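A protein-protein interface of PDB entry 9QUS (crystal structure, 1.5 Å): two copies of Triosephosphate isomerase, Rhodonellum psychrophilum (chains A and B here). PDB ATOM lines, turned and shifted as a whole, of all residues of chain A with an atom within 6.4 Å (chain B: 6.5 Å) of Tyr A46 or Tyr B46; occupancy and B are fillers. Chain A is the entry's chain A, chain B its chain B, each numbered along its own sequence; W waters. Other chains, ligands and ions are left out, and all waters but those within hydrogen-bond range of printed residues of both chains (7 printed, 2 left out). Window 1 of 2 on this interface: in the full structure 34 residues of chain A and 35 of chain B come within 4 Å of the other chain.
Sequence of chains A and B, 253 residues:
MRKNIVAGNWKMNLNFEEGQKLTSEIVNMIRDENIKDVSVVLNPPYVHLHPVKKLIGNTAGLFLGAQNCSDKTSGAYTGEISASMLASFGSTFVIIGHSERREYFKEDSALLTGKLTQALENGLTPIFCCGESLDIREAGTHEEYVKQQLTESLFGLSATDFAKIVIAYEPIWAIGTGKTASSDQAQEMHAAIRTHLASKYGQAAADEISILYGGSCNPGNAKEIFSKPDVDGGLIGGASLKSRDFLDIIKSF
The side-chain amide oxygen (OE1) of Gln A67 sits at hydrogen-bond distance from the backbone NH (N) of Gly B79, at 2.8 Å. The side-chain amide oxygen of Gln B67 lies within hydrogen-bond range of the backbone NH of Gly A79, 2.7 Å away. ND1 of His A50 is in hydrogen-bond range of ND1 of His B50, at 3.1 Å. The side-chain carboxylate (OE2) of Glu A80 is in salt-bridge range of the guanidinium group (NH1) of Arg B101 (2.7 Å). The guanidinium group (NH1) of Arg A101 is in salt-bridge range of the side-chain carboxylate (OE2) of Glu B80, 2.8 Å away.
The backbone carbonyl oxygen (O) of Ile A81 sits at hydrogen-bond distance from the backbone NH (N) of Ser A70 (2.7 Å). NE of Arg B101 lies close to ND2 of Asn B68, at 3.2 Å. O of Ile B81 sits at hydrogen-bond distance from N of Ser B70, 2.7 Å away. OH of Tyr B46 lies within hydrogen-bond range of O of Asn B68.
Among the printed residues, pairs that only touch across the chains: Gly A79 with Tyr B46, Tyr A46 with Tyr B46, Tyr A46 with Gly B79, Met A85 with Pro B45, Ile A81 with Pro B45, Pro A45 with Ile B81, Ile A81 with Tyr B46, Pro A45 with Met B85, Tyr A46 with Ile B81, Gly A79 with Arg B101, Tyr A46 with Val B47, Val A47 with Tyr B46, Leu A49 with Val B47, Arg A101 with Gly B79, Val A47 with Leu B49 and Ile A81 with Val B47.
Of chain B, only Tyr B46 (3.3 Å), Val B47 (3.7 Å), Gly B79 (3.3 Å) and Ile B81 (3.6 Å) come within 4 Å of Tyr A46. Tyr B46 touches four residues of chain A. Of the printed residues of chain A, Ile B81 touches Pro A45 and Tyr A46. Of the printed residues of chain A, Glu B80 touches Arg A101 (2.8 Å). Printed residues of chain B within 4 Å of His A50: His B50. Ala B66 touches none of the printed residues of chain A. The nearest residue of chain A that does not touch Tyr B46 is Glu A80 (5.5 Å). The nearest printed residue of chain B that does not touch Met A85 is Val B47 (4.2 Å).
Of the 19 printed residues of chain B, 11 touch a printed residue of chain A. Printed residues of chain B that touch a printed residue of chain A: Pro B45, Tyr B46, Val B47, Leu B49, His B50, Gln B67, Gly B79, Glu B80, Ile B81, Met B85 and Arg B101. Hydrophobic or aromatic side chains of chain B within 4 Å of the printed part of chain A: Pro B45, Tyr B46, Val B47, Leu B49, His B50, Ile B81 and Met B85. Along chain B the printed residues that touch a printed residue of chain A span positions 45 to 101. Hydrophobic or aromatic side chains of chain A within 4 Å of the printed part of chain B: Pro A45, Tyr A46, Val A47, Leu A49, His A50, Ile A81 and Met A85. Among the printed residues, 21 pairs touch across the chains.
Pro A45 touches Met B85, and with the chains exchanged Met A85 touches Pro B45. Tyr A46 touches Gly B79, and with the chains exchanged Gly A79 touches Tyr B46. Glu A80 touches Arg B101, and with the chains exchanged Arg A101 touches Glu B80. 18 positions are printed for both chains.
Water W1 lies within hydrogen-bond range of O of Glu B80 (2.6 Å) and OE1 of Gln A67 (3.1 Å). Water W5 bridges the side-chain amide oxygen of Gln B67 (2.8 Å) and the backbone carbonyl oxygen of Glu A80 (2.9 Å). Water W4 bridges N of Tyr A46 (3.2 Å) and O of Gly B79 (3.4 Å).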
ATOM      1  N   PRO A  44      -0.740  -1.063 -27.976  1.00  0.00           N
ATOM      2  CA  PRO A  44      -1.302   0.254 -28.279  1.00  0.00           C
ATOM      3  C   PRO A  44      -1.902   0.875 -27.030  1.00  0.00           C
ATOM      4  O   PRO A  44      -2.019   0.212 -25.989  1.00  0.00           O
ATOM      5  CB  PRO A  44      -2.386  -0.056 -29.319  1.00  0.00           C
ATOM      6  CG  PRO A  44      -2.906  -1.398 -28.860  1.00  0.00           C
ATOM      7  CD  PRO A  44      -1.686  -2.149 -28.307  1.00  0.00           C
ATOM      8  N   PRO A  45      -2.300   2.143 -27.103  1.00  0.00           N
ATOM      9  CA  PRO A  45      -3.035   2.744 -25.983  1.00  0.00           C
ATOM     10  C   PRO A  45      -4.298   1.955 -25.665  1.00  0.00           C
ATOM     11  O   PRO A  45      -4.795   1.165 -26.472  1.00  0.00           O
ATOM     12  CB  PRO A  45      -3.365   4.155 -26.487  1.00  0.00           C
ATOM     13  CG  PRO A  45      -2.316   4.439 -27.531  1.00  0.00           C
ATOM     14  CD  PRO A  45      -2.018   3.108 -28.180  1.00  0.00           C
ATOM     15  N   TYR A  46      -4.814   2.182 -24.451  1.00  0.00           N
ATOM     16  CA  TYR A  46      -5.978   1.437 -23.977  1.00  0.00           C
ATOM     17  C   TYR A  46      -7.113   1.459 -24.992  1.00  0.00           C
ATOM     18  O   TYR A  46      -7.790   0.448 -25.211  1.00  0.00           O
ATOM     19  CB  TYR A  46      -6.492   2.019 -22.656  1.00  0.00           C
ATOM     20  CG  TYR A  46      -5.542   1.954 -21.488  1.00  0.00           C
ATOM     21  CD1 TYR A  46      -5.060   0.739 -21.033  1.00  0.00           C
ATOM     22  CD2 TYR A  46      -5.170   3.107 -20.807  1.00  0.00           C
ATOM     23  CE1 TYR A  46      -4.204   0.673 -19.956  1.00  0.00           C
ATOM     24  CE2 TYR A  46      -4.319   3.055 -19.729  1.00  0.00           C
ATOM     25  CZ  TYR A  46      -3.837   1.834 -19.305  1.00  0.00           C
ATOM     26  OH  TYR A  46      -2.982   1.771 -18.227  1.00  0.00           O
ATOM     27  N   VAL A  47      -7.364   2.624 -25.592  1.00  0.00           N
ATOM     28  CA  VAL A  47      -8.578   2.809 -26.378  1.00  0.00           C
ATOM     29  C   VAL A  47      -8.579   1.924 -27.616  1.00  0.00           C
ATOM     30  O   VAL A  47      -9.648   1.580 -28.140  1.00  0.00           O
ATOM     31  CB  VAL A  47      -8.738   4.298 -26.747  1.00  0.00           C
ATOM     32  CG1 VAL A  47      -9.078   5.124 -25.512  1.00  0.00           C
ATOM     33  CG2 VAL A  47      -7.462   4.824 -27.396  1.00  0.00           C
ATOM     34  N   HIS A  48      -7.402   1.529 -28.100  1.00  0.00           N
ATOM     35  CA  HIS A  48      -7.316   0.778 -29.346  1.00  0.00           C
ATOM     36  C   HIS A  48      -7.511  -0.723 -29.172  1.00  0.00           C
ATOM     37  O   HIS A  48      -7.692  -1.420 -30.175  1.00  0.00           O
ATOM     38  CB  HIS A  48      -5.955   0.979 -30.027  1.00  0.00           C
ATOM     39  CG  HIS A  48      -5.679   2.384 -30.459  1.00  0.00           C
ATOM     40  ND1 HIS A  48      -5.128   3.326 -29.618  1.00  0.00           N
ATOM     41  CD2 HIS A  48      -5.857   3.000 -31.650  1.00  0.00           C
ATOM     42  CE1 HIS A  48      -4.990   4.466 -30.269  1.00  0.00           C
ATOM     43  NE2 HIS A  48      -5.421   4.294 -31.507  1.00  0.00           N
ATOM     44  N   LEU A  49      -7.433  -1.242 -27.945  1.00  0.00           N
ATOM     45  CA  LEU A  49      -7.349  -2.687 -27.756  1.00  0.00           C
ATOM     46  C   LEU A  49      -8.479  -3.414 -28.478  1.00  0.00           C
ATOM     47  O   LEU A  49      -8.252  -4.409 -29.175  1.00  0.00           O
ATOM     48  CB  LEU A  49      -7.377  -3.023 -26.263  1.00  0.00           C
ATOM     49  CG  LEU A  49      -6.296  -2.436 -25.358  1.00  0.00           C
ATOM     50  CD1 LEU A  49      -6.530  -2.900 -23.922  1.00  0.00           C
ATOM     51  CD2 LEU A  49      -4.904  -2.835 -25.826  1.00  0.00           C
ATOM     52  N   HIS A  50      -9.708  -2.932 -28.314  1.00  0.00           N
ATOM     53  CA  HIS A  50     -10.856  -3.653 -28.864  1.00  0.00           C
ATOM     54  C   HIS A  50     -10.809  -3.758 -30.381  1.00  0.00           C
ATOM     55  O   HIS A  50     -10.962  -4.876 -30.906  1.00  0.00           O
ATOM     56  CB  HIS A  50     -12.150  -2.984 -28.386  1.00  0.00           C
ATOM     57  CG  HIS A  50     -13.397  -3.668 -28.859  1.00  0.00           C
ATOM     58  ND1 HIS A  50     -14.068  -3.282 -29.999  1.00  0.00           N
ATOM     59  CD2 HIS A  50     -14.097  -4.706 -28.343  1.00  0.00           C
ATOM     60  CE1 HIS A  50     -15.126  -4.056 -30.168  1.00  0.00           C
ATOM     61  NE2 HIS A  50     -15.168  -4.926 -29.176  1.00  0.00           N
ATOM     62  N   ALA A  66      -0.611  -4.201 -23.824  1.00  0.00           N
ATOM     63  CA  ALA A  66      -1.076  -2.960 -23.225  1.00  0.00           C
ATOM     64  C   ALA A  66       0.143  -2.289 -22.609  1.00  0.00           C
ATOM     65  O   ALA A  66       1.183  -2.924 -22.413  1.00  0.00           O
ATOM     66  CB  ALA A  66      -2.173  -3.204 -22.182  1.00  0.00           C
ATOM     67  N   GLN A  67      -0.002  -1.008 -22.282  1.00  0.00           N
ATOM     68  CA  GLN A  67       1.126  -0.209 -21.823  1.00  0.00           C
ATOM     69  C   GLN A  67       1.171  -0.017 -20.313  1.00  0.00           C
ATOM     70  O   GLN A  67       2.155   0.535 -19.809  1.00  0.00           O
ATOM     71  CB  GLN A  67       1.108   1.162 -22.507  1.00  0.00           C
ATOM     72  CG  GLN A  67       1.332   1.083 -24.009  1.00  0.00           C
ATOM     73  CD  GLN A  67       1.348   2.445 -24.684  1.00  0.00           C
ATOM     74  OE1 GLN A  67       1.563   3.472 -24.040  1.00  0.00           O
ATOM     75  NE2 GLN A  67       1.115   2.455 -25.991  1.00  0.00           N
ATOM     76  N   ASN A  68       0.167  -0.492 -19.581  1.00  0.00           N
ATOM     77  CA  ASN A  68       0.103  -0.302 -18.138  1.00  0.00           C
ATOM     78  C   ASN A  68      -1.165  -0.974 -17.634  1.00  0.00           C
ATOM     79  O   ASN A  68      -2.079  -1.273 -18.409  1.00  0.00           O
ATOM     80  CB  ASN A  68       0.117   1.188 -17.765  1.00  0.00           C
ATOM     81  CG  ASN A  68       0.116   1.419 -16.260  1.00  0.00           C
ATOM     82  OD1 ASN A  68       0.785   0.707 -15.507  1.00  0.00           O
ATOM     83  ND2 ASN A  68      -0.648   2.415 -15.815  1.00  0.00           N
ATOM     84  N   CYS A  69      -1.202  -1.231 -16.328  1.00  0.00           N
ATOM     85  CA  CYS A  69      -2.412  -1.709 -15.680  1.00  0.00           C
ATOM     86  C   CYS A  69      -2.370  -1.307 -14.214  1.00  0.00           C
ATOM     87  O   CYS A  69      -1.312  -0.989 -13.665  1.00  0.00           O
ATOM     88  CB  CYS A  69      -2.568  -3.227 -15.823  1.00  0.00           C
ATOM     89  SG  CYS A  69      -1.335  -4.197 -14.913  1.00  0.00           S
ATOM     90  N   SER A  70      -3.539  -1.330 -13.583  1.00  0.00           N
ATOM     91  CA  SER A  70      -3.653  -0.927 -12.192  1.00  0.00           C
ATOM     92  C   SER A  70      -3.128  -2.018 -11.268  1.00  0.00           C
ATOM     93  O   SER A  70      -3.115  -3.205 -11.614  1.00  0.00           O
ATOM     94  CB  SER A  70      -5.109  -0.615 -11.847  1.00  0.00           C
ATOM     95  OG  SER A  70      -5.235  -0.190 -10.503  1.00  0.00           O
ATOM     96  N   GLY A  79     -10.199   6.695 -13.994  1.00  0.00           N
ATOM     97  CA  GLY A  79      -9.142   6.817 -14.970  1.00  0.00           C
ATOM     98  C   GLY A  79      -8.275   5.590 -15.150  1.00  0.00           C
ATOM     99  O   GLY A  79      -7.554   5.505 -16.153  1.00  0.00           O
ATOM    100  N   GLU A  80      -8.332   4.636 -14.226  1.00  0.00           N
ATOM    101  CA  GLU A  80      -7.415   3.507 -14.212  1.00  0.00           C
ATOM    102  C   GLU A  80      -8.033   2.288 -14.884  1.00  0.00           C
ATOM    103  O   GLU A  80      -9.255   2.120 -14.922  1.00  0.00           O
ATOM    104  CB  GLU A  80      -7.006   3.160 -12.779  1.00  0.00           C
ATOM    105  CG  GLU A  80      -6.224   4.265 -12.096  1.00  0.00           C
ATOM    106  CD  GLU A  80      -4.954   4.603 -12.842  1.00  0.00           C
ATOM    107  OE1 GLU A  80      -4.060   3.738 -12.922  1.00  0.00           O
ATOM    108  OE2 GLU A  80      -4.853   5.732 -13.360  1.00  0.00           O
ATOM    109  N   ILE A  81      -7.160   1.434 -15.412  1.00  0.00           N
ATOM    110  CA  ILE A  81      -7.549   0.242 -16.154  1.00  0.00           C
ATOM    111  C   ILE A  81      -6.957  -0.975 -15.455  1.00  0.00           C
ATOM    112  O   ILE A  81      -5.762  -0.995 -15.140  1.00  0.00           O
ATOM    113  CB  ILE A  81      -7.073   0.313 -17.616  1.00  0.00           C
ATOM    114  CG1 ILE A  81      -7.613   1.574 -18.296  1.00  0.00           C
ATOM    115  CG2 ILE A  81      -7.494  -0.942 -18.374  1.00  0.00           C
ATOM    116  CD1 ILE A  81      -9.124   1.632 -18.383  1.00  0.00           C
ATOM    117  N   MET A  85      -9.831  -6.137 -16.996  1.00  0.00           N
ATOM    118  CA  MET A  85     -10.295  -5.404 -18.169  1.00  0.00           C
ATOM    119  C   MET A  85      -9.450  -5.748 -19.389  1.00  0.00           C
ATOM    120  O   MET A  85      -9.978  -6.106 -20.447  1.00  0.00           O
ATOM    121  CB  MET A  85     -10.253  -3.897 -17.905  1.00  0.00           C
ATOM    122  CG  MET A  85     -11.446  -3.358 -17.146  1.00  0.00           C
ATOM    123  SD  MET A  85     -11.306  -1.587 -16.853  1.00  0.00           S
ATOM    124  CE  MET A  85     -12.521  -1.373 -15.560  1.00  0.00           C
ATOM    125  N   LEU A  86      -8.126  -5.641 -19.256  1.00  0.00           N
ATOM    126  CA  LEU A  86      -7.242  -5.942 -20.376  1.00  0.00           C
ATOM    127  C   LEU A  86      -7.473  -7.358 -20.889  1.00  0.00           C
ATOM    128  O   LEU A  86      -7.687  -7.567 -22.088  1.00  0.00           O
ATOM    129  CB  LEU A  86      -5.786  -5.748 -19.956  1.00  0.00           C
ATOM    130  CG  LEU A  86      -5.398  -4.327 -19.542  1.00  0.00           C
ATOM    131  CD1 LEU A  86      -3.950  -4.276 -19.072  1.00  0.00           C
ATOM    132  CD2 LEU A  86      -5.619  -3.349 -20.692  1.00  0.00           C
ATOM    133  N   ARG A 101       6.748   5.884 -16.999  1.00  0.00           N
ATOM    134  CA  ARG A 101       5.812   5.898 -15.882  1.00  0.00           C
ATOM    135  C   ARG A 101       6.527   6.014 -14.544  1.00  0.00           C
ATOM    136  O   ARG A 101       6.051   6.728 -13.654  1.00  0.00           O
ATOM    137  CB  ARG A 101       4.942   4.643 -15.913  1.00  0.00           C
ATOM    138  CG  ARG A 101       4.066   4.544 -17.166  1.00  0.00           C
ATOM    139  CD  ARG A 101       2.774   3.794 -16.891  1.00  0.00           C
ATOM    140  NE  ARG A 101       1.960   4.471 -15.887  1.00  0.00           N
ATOM    141  CZ  ARG A 101       1.173   5.508 -16.135  1.00  0.00           C
ATOM    142  NH1 ARG A 101       1.066   6.020 -17.349  1.00  0.00           N
ATOM    143  NH2 ARG A 101       0.475   6.046 -15.137  1.00  0.00           N
ATOM    144  N   PRO B  44     -17.157   5.451 -19.298  1.00  0.00           N
ATOM    145  CA  PRO B  44     -16.576   4.149 -18.956  1.00  0.00           C
ATOM    146  C   PRO B  44     -15.063   4.208 -19.022  1.00  0.00           C
ATOM    147  O   PRO B  44     -14.489   5.202 -19.496  1.00  0.00           O
ATOM    148  CB  PRO B  44     -17.145   3.216 -20.035  1.00  0.00           C
ATOM    149  CG  PRO B  44     -17.221   4.119 -21.242  1.00  0.00           C
ATOM    150  CD  PRO B  44     -17.584   5.512 -20.710  1.00  0.00           C
ATOM    151  N   PRO B  45     -14.380   3.167 -18.554  1.00  0.00           N
ATOM    152  CA  PRO B  45     -12.922   3.113 -18.712  1.00  0.00           C
ATOM    153  C   PRO B  45     -12.520   3.242 -20.174  1.00  0.00           C
ATOM    154  O   PRO B  45     -13.310   3.000 -21.090  1.00  0.00           O
ATOM    155  CB  PRO B  45     -12.544   1.737 -18.153  1.00  0.00           C
ATOM    156  CG  PRO B  45     -13.671   1.378 -17.220  1.00  0.00           C
ATOM    157  CD  PRO B  45     -14.917   2.022 -17.795  1.00  0.00           C
ATOM    158  N   TYR B  46     -11.254   3.622 -20.380  1.00  0.00           N
ATOM    159  CA  TYR B  46     -10.744   3.854 -21.731  1.00  0.00           C
ATOM    160  C   TYR B  46     -11.082   2.696 -22.662  1.00  0.00           C
ATOM    161  O   TYR B  46     -11.520   2.898 -23.801  1.00  0.00           O
ATOM    162  CB  TYR B  46      -9.225   4.034 -21.710  1.00  0.00           C
ATOM    163  CG  TYR B  46      -8.689   5.240 -20.983  1.00  0.00           C
ATOM    164  CD1 TYR B  46      -9.138   6.516 -21.275  1.00  0.00           C
ATOM    165  CD2 TYR B  46      -7.703   5.098 -20.017  1.00  0.00           C
ATOM    166  CE1 TYR B  46      -8.626   7.616 -20.615  1.00  0.00           C
ATOM    167  CE2 TYR B  46      -7.189   6.184 -19.353  1.00  0.00           C
ATOM    168  CZ  TYR B  46      -7.653   7.442 -19.652  1.00  0.00           C
ATOM    169  OH  TYR B  46      -7.139   8.531 -18.987  1.00  0.00           O
ATOM    170  N   VAL B  47     -10.854   1.467 -22.197  1.00  0.00           N
ATOM    171  CA  VAL B  47     -10.962   0.304 -23.065  1.00  0.00           C
ATOM    172  C   VAL B  47     -12.373   0.128 -23.605  1.00  0.00           C
ATOM    173  O   VAL B  47     -12.569  -0.539 -24.629  1.00  0.00           O
ATOM    174  CB  VAL B  47     -10.506  -0.958 -22.303  1.00  0.00           C
ATOM    175  CG1 VAL B  47      -9.022  -0.891 -21.988  1.00  0.00           C
ATOM    176  CG2 VAL B  47     -11.317  -1.123 -21.013  1.00  0.00           C
ATOM    177  N   HIS B  48     -13.368   0.725 -22.951  1.00  0.00           N
ATOM    178  CA  HIS B  48     -14.757   0.522 -23.338  1.00  0.00           C
ATOM    179  C   HIS B  48     -15.253   1.510 -24.386  1.00  0.00           C
ATOM    180  O   HIS B  48     -16.307   1.269 -24.986  1.00  0.00           O
ATOM    181  CB  HIS B  48     -15.674   0.634 -22.115  1.00  0.00           C
ATOM    182  CG  HIS B  48     -15.496  -0.464 -21.117  1.00  0.00           C
ATOM    183  ND1 HIS B  48     -16.183  -1.653 -21.197  1.00  0.00           N
ATOM    184  CD2 HIS B  48     -14.716  -0.553 -20.013  1.00  0.00           C
ATOM    185  CE1 HIS B  48     -15.836  -2.430 -20.188  1.00  0.00           C
ATOM    186  NE2 HIS B  48     -14.946  -1.786 -19.454  1.00  0.00           N
ATOM    187  N   LEU B  49     -14.528   2.605 -24.622  1.00  0.00           N
ATOM    188  CA  LEU B  49     -15.079   3.708 -25.403  1.00  0.00           C
ATOM    189  C   LEU B  49     -15.530   3.241 -26.781  1.00  0.00           C
ATOM    190  O   LEU B  49     -16.622   3.592 -27.240  1.00  0.00           O
ATOM    191  CB  LEU B  49     -14.043   4.826 -25.523  1.00  0.00           C
ATOM    192  CG  LEU B  49     -13.580   5.422 -24.194  1.00  0.00           C
ATOM    193  CD1 LEU B  49     -12.505   6.476 -24.421  1.00  0.00           C
ATOM    194  CD2 LEU B  49     -14.763   6.021 -23.430  1.00  0.00           C
ATOM    195  N   HIS B  50     -14.709   2.434 -27.450  1.00  0.00           N
ATOM    196  CA  HIS B  50     -15.037   2.032 -28.819  1.00  0.00           C
ATOM    197  C   HIS B  50     -16.330   1.228 -28.892  1.00  0.00           C
ATOM    198  O   HIS B  50     -17.235   1.614 -29.650  1.00  0.00           O
ATOM    199  CB  HIS B  50     -13.861   1.259 -29.419  1.00  0.00           C
ATOM    200  CG  HIS B  50     -14.105   0.776 -30.817  1.00  0.00           C
ATOM    201  ND1 HIS B  50     -14.695  -0.439 -31.095  1.00  0.00           N
ATOM    202  CD2 HIS B  50     -13.837   1.345 -32.016  1.00  0.00           C
ATOM    203  CE1 HIS B  50     -14.780  -0.596 -32.404  1.00  0.00           C
ATOM    204  NE2 HIS B  50     -14.265   0.470 -32.986  1.00  0.00           N
ATOM    205  N   PRO B  51     -16.482   0.118 -28.164  1.00  0.00           N
ATOM    206  CA  PRO B  51     -17.756  -0.622 -28.246  1.00  0.00           C
ATOM    207  C   PRO B  51     -18.929   0.123 -27.632  1.00  0.00           C
ATOM    208  O   PRO B  51     -20.056  -0.006 -28.126  1.00  0.00           O
ATOM    209  CB  PRO B  51     -17.460  -1.930 -27.497  1.00  0.00           C
ATOM    210  CG  PRO B  51     -16.328  -1.594 -26.575  1.00  0.00           C
ATOM    211  CD  PRO B  51     -15.494  -0.563 -27.308  1.00  0.00           C
ATOM    212  N   ALA B  66     -15.239  10.170 -20.871  1.00  0.00           N
ATOM    213  CA  ALA B  66     -13.999   9.508 -20.509  1.00  0.00           C
ATOM    214  C   ALA B  66     -13.644   9.990 -19.114  1.00  0.00           C
ATOM    215  O   ALA B  66     -14.128  11.033 -18.667  1.00  0.00           O
ATOM    216  CB  ALA B  66     -12.890   9.820 -21.504  1.00  0.00           C
ATOM    217  N   GLN B  67     -12.775   9.233 -18.440  1.00  0.00           N
ATOM    218  CA  GLN B  67     -12.477   9.465 -17.034  1.00  0.00           C
ATOM    219  C   GLN B  67     -11.206  10.272 -16.808  1.00  0.00           C
ATOM    220  O   GLN B  67     -10.950  10.678 -15.671  1.00  0.00           O
ATOM    221  CB  GLN B  67     -12.375   8.121 -16.292  1.00  0.00           C
ATOM    222  CG  GLN B  67     -13.690   7.358 -16.252  1.00  0.00           C
ATOM    223  CD  GLN B  67     -13.586   6.032 -15.506  1.00  0.00           C
ATOM    224  OE1 GLN B  67     -12.643   5.803 -14.752  1.00  0.00           O
ATOM    225  NE2 GLN B  67     -14.552   5.150 -15.726  1.00  0.00           N
ATOM    226  N   ASN B  68     -10.419  10.534 -17.850  1.00  0.00           N
ATOM    227  CA  ASN B  68      -9.166  11.264 -17.704  1.00  0.00           C
ATOM    228  C   ASN B  68      -8.544  11.420 -19.082  1.00  0.00           C
ATOM    229  O   ASN B  68      -8.878  10.690 -20.020  1.00  0.00           O
ATOM    230  CB  ASN B  68      -8.203  10.540 -16.755  1.00  0.00           C
ATOM    231  CG  ASN B  68      -6.923  11.312 -16.512  1.00  0.00           C
ATOM    232  OD1 ASN B  68      -6.937  12.535 -16.381  1.00  0.00           O
ATOM    233  ND2 ASN B  68      -5.803  10.598 -16.461  1.00  0.00           N
ATOM    234  N   CYS B  69      -7.641  12.392 -19.194  1.00  0.00           N
ATOM    235  CA  CYS B  69      -6.874  12.582 -20.416  1.00  0.00           C
ATOM    236  C   CYS B  69      -5.554  13.255 -20.071  1.00  0.00           C
ATOM    237  O   CYS B  69      -5.410  13.895 -19.026  1.00  0.00           O
ATOM    238  CB  CYS B  69      -7.653  13.410 -21.443  1.00  0.00           C
ATOM    239  SG  CYS B  69      -7.774  15.178 -21.071  1.00  0.00           S
ATOM    240  N   SER B  70      -4.589  13.104 -20.972  1.00  0.00           N
ATOM    241  CA  SER B  70      -3.263  13.667 -20.763  1.00  0.00           C
ATOM    242  C   SER B  70      -3.292  15.181 -20.928  1.00  0.00           C
ATOM    243  O   SER B  70      -4.150  15.738 -21.618  1.00  0.00           O
ATOM    244  CB  SER B  70      -2.272  13.054 -21.753  1.00  0.00           C
ATOM    245  OG  SER B  70      -0.949  13.484 -21.497  1.00  0.00           O
ATOM    246  N   GLY B  79       1.379   4.567 -21.487  1.00  0.00           N
ATOM    247  CA  GLY B  79       0.262   4.341 -20.597  1.00  0.00           C
ATOM    248  C   GLY B  79      -0.772   5.446 -20.559  1.00  0.00           C
ATOM    249  O   GLY B  79      -1.831   5.259 -19.945  1.00  0.00           O
ATOM    250  N   GLU B  80      -0.507   6.579 -21.197  1.00  0.00           N
ATOM    251  CA  GLU B  80      -1.383   7.738 -21.149  1.00  0.00           C
ATOM    252  C   GLU B  80      -2.234   7.828 -22.411  1.00  0.00           C
ATOM    253  O   GLU B  80      -1.886   7.298 -23.469  1.00  0.00           O
ATOM    254  CB  GLU B  80      -0.562   9.017 -20.973  1.00  0.00           C
ATOM    255  CG  GLU B  80       0.200   9.055 -19.663  1.00  0.00           C
ATOM    256  CD  GLU B  80      -0.724   9.018 -18.463  1.00  0.00           C
ATOM    257  OE1 GLU B  80      -1.304  10.070 -18.125  1.00  0.00           O
ATOM    258  OE2 GLU B  80      -0.878   7.933 -17.866  1.00  0.00           O
ATOM    259  N   ILE B  81      -3.363   8.521 -22.276  1.00  0.00           N
ATOM    260  CA  ILE B  81      -4.349   8.677 -23.339  1.00  0.00           C
ATOM    261  C   ILE B  81      -4.522  10.166 -23.597  1.00  0.00           C
ATOM    262  O   ILE B  81      -4.734  10.940 -22.656  1.00  0.00           O
ATOM    263  CB  ILE B  81      -5.696   8.027 -22.967  1.00  0.00           C
ATOM    264  CG1 ILE B  81      -5.505   6.537 -22.666  1.00  0.00           C
ATOM    265  CG2 ILE B  81      -6.714   8.235 -24.087  1.00  0.00           C
ATOM    266  CD1 ILE B  81      -5.035   5.718 -23.850  1.00  0.00           C
ATOM    267  N   MET B  85      -6.999  11.331 -28.990  1.00  0.00           N
ATOM    268  CA  MET B  85      -7.425   9.936 -29.043  1.00  0.00           C
ATOM    269  C   MET B  85      -8.886   9.801 -28.635  1.00  0.00           C
ATOM    270  O   MET B  85      -9.668   9.110 -29.297  1.00  0.00           O
ATOM    271  CB  MET B  85      -6.544   9.078 -28.132  1.00  0.00           C
ATOM    272  CG  MET B  85      -5.105   8.919 -28.576  1.00  0.00           C
ATOM    273  SD  MET B  85      -4.191   7.887 -27.407  1.00  0.00           S
ATOM    274  CE  MET B  85      -2.554   7.915 -28.126  1.00  0.00           C
ATOM    275  N   LEU B  86      -9.266  10.439 -27.526  1.00  0.00           N
ATOM    276  CA  LEU B  86     -10.641  10.340 -27.047  1.00  0.00           C
ATOM    277  C   LEU B  86     -11.624  10.823 -28.105  1.00  0.00           C
ATOM    278  O   LEU B  86     -12.571  10.111 -28.459  1.00  0.00           O
ATOM    279  CB  LEU B  86     -10.798  11.135 -25.752  1.00  0.00           C
ATOM    280  CG  LEU B  86      -9.979  10.610 -24.572  1.00  0.00           C
ATOM    281  CD1 LEU B  86     -10.116  11.529 -23.364  1.00  0.00           C
ATOM    282  CD2 LEU B  86     -10.387   9.191 -24.212  1.00  0.00           C
ATOM    283  N   ARG B 101      -8.147  11.028  -8.636  1.00  0.00           N
ATOM    284  CA  ARG B 101      -6.889  11.247  -9.342  1.00  0.00           C
ATOM    285  C   ARG B 101      -6.034  12.299  -8.648  1.00  0.00           C
ATOM    286  O   ARG B 101      -4.814  12.135  -8.542  1.00  0.00           O
ATOM    287  CB  ARG B 101      -7.163  11.648 -10.792  1.00  0.00           C
ATOM    288  CG  ARG B 101      -7.868  10.568 -11.589  1.00  0.00           C
ATOM    289  CD  ARG B 101      -7.499  10.610 -13.066  1.00  0.00           C
ATOM    290  NE  ARG B 101      -6.077  10.365 -13.278  1.00  0.00           N
ATOM    291  CZ  ARG B 101      -5.522   9.163 -13.284  1.00  0.00           C
ATOM    292  NH1 ARG B 101      -6.237   8.070 -13.071  1.00  0.00           N
ATOM    293  NH2 ARG B 101      -4.217   9.053 -13.512  1.00  0.00           N
HETATM  294  O   HOH W   1      -1.227   4.846 -23.928  1.00  0.00           O
HETATM  295  O   HOH W   2      -3.083   6.523 -16.093  1.00  0.00           O
HETATM  296  O   HOH W   3      -5.474   7.444 -16.708  1.00  0.00           O
HETATM  297  O   HOH W   4      -2.517   2.979 -22.354  1.00  0.00           O
HETATM  298  O   HOH W   5     -11.255   3.873 -16.181  1.00  0.00           O
HETATM  299  O   HOH W   6     -10.275   5.239 -17.992  1.00  0.00           O
HETATM  300  O   HOH W   7      -2.424   4.373 -17.770  1.00  0.00           O
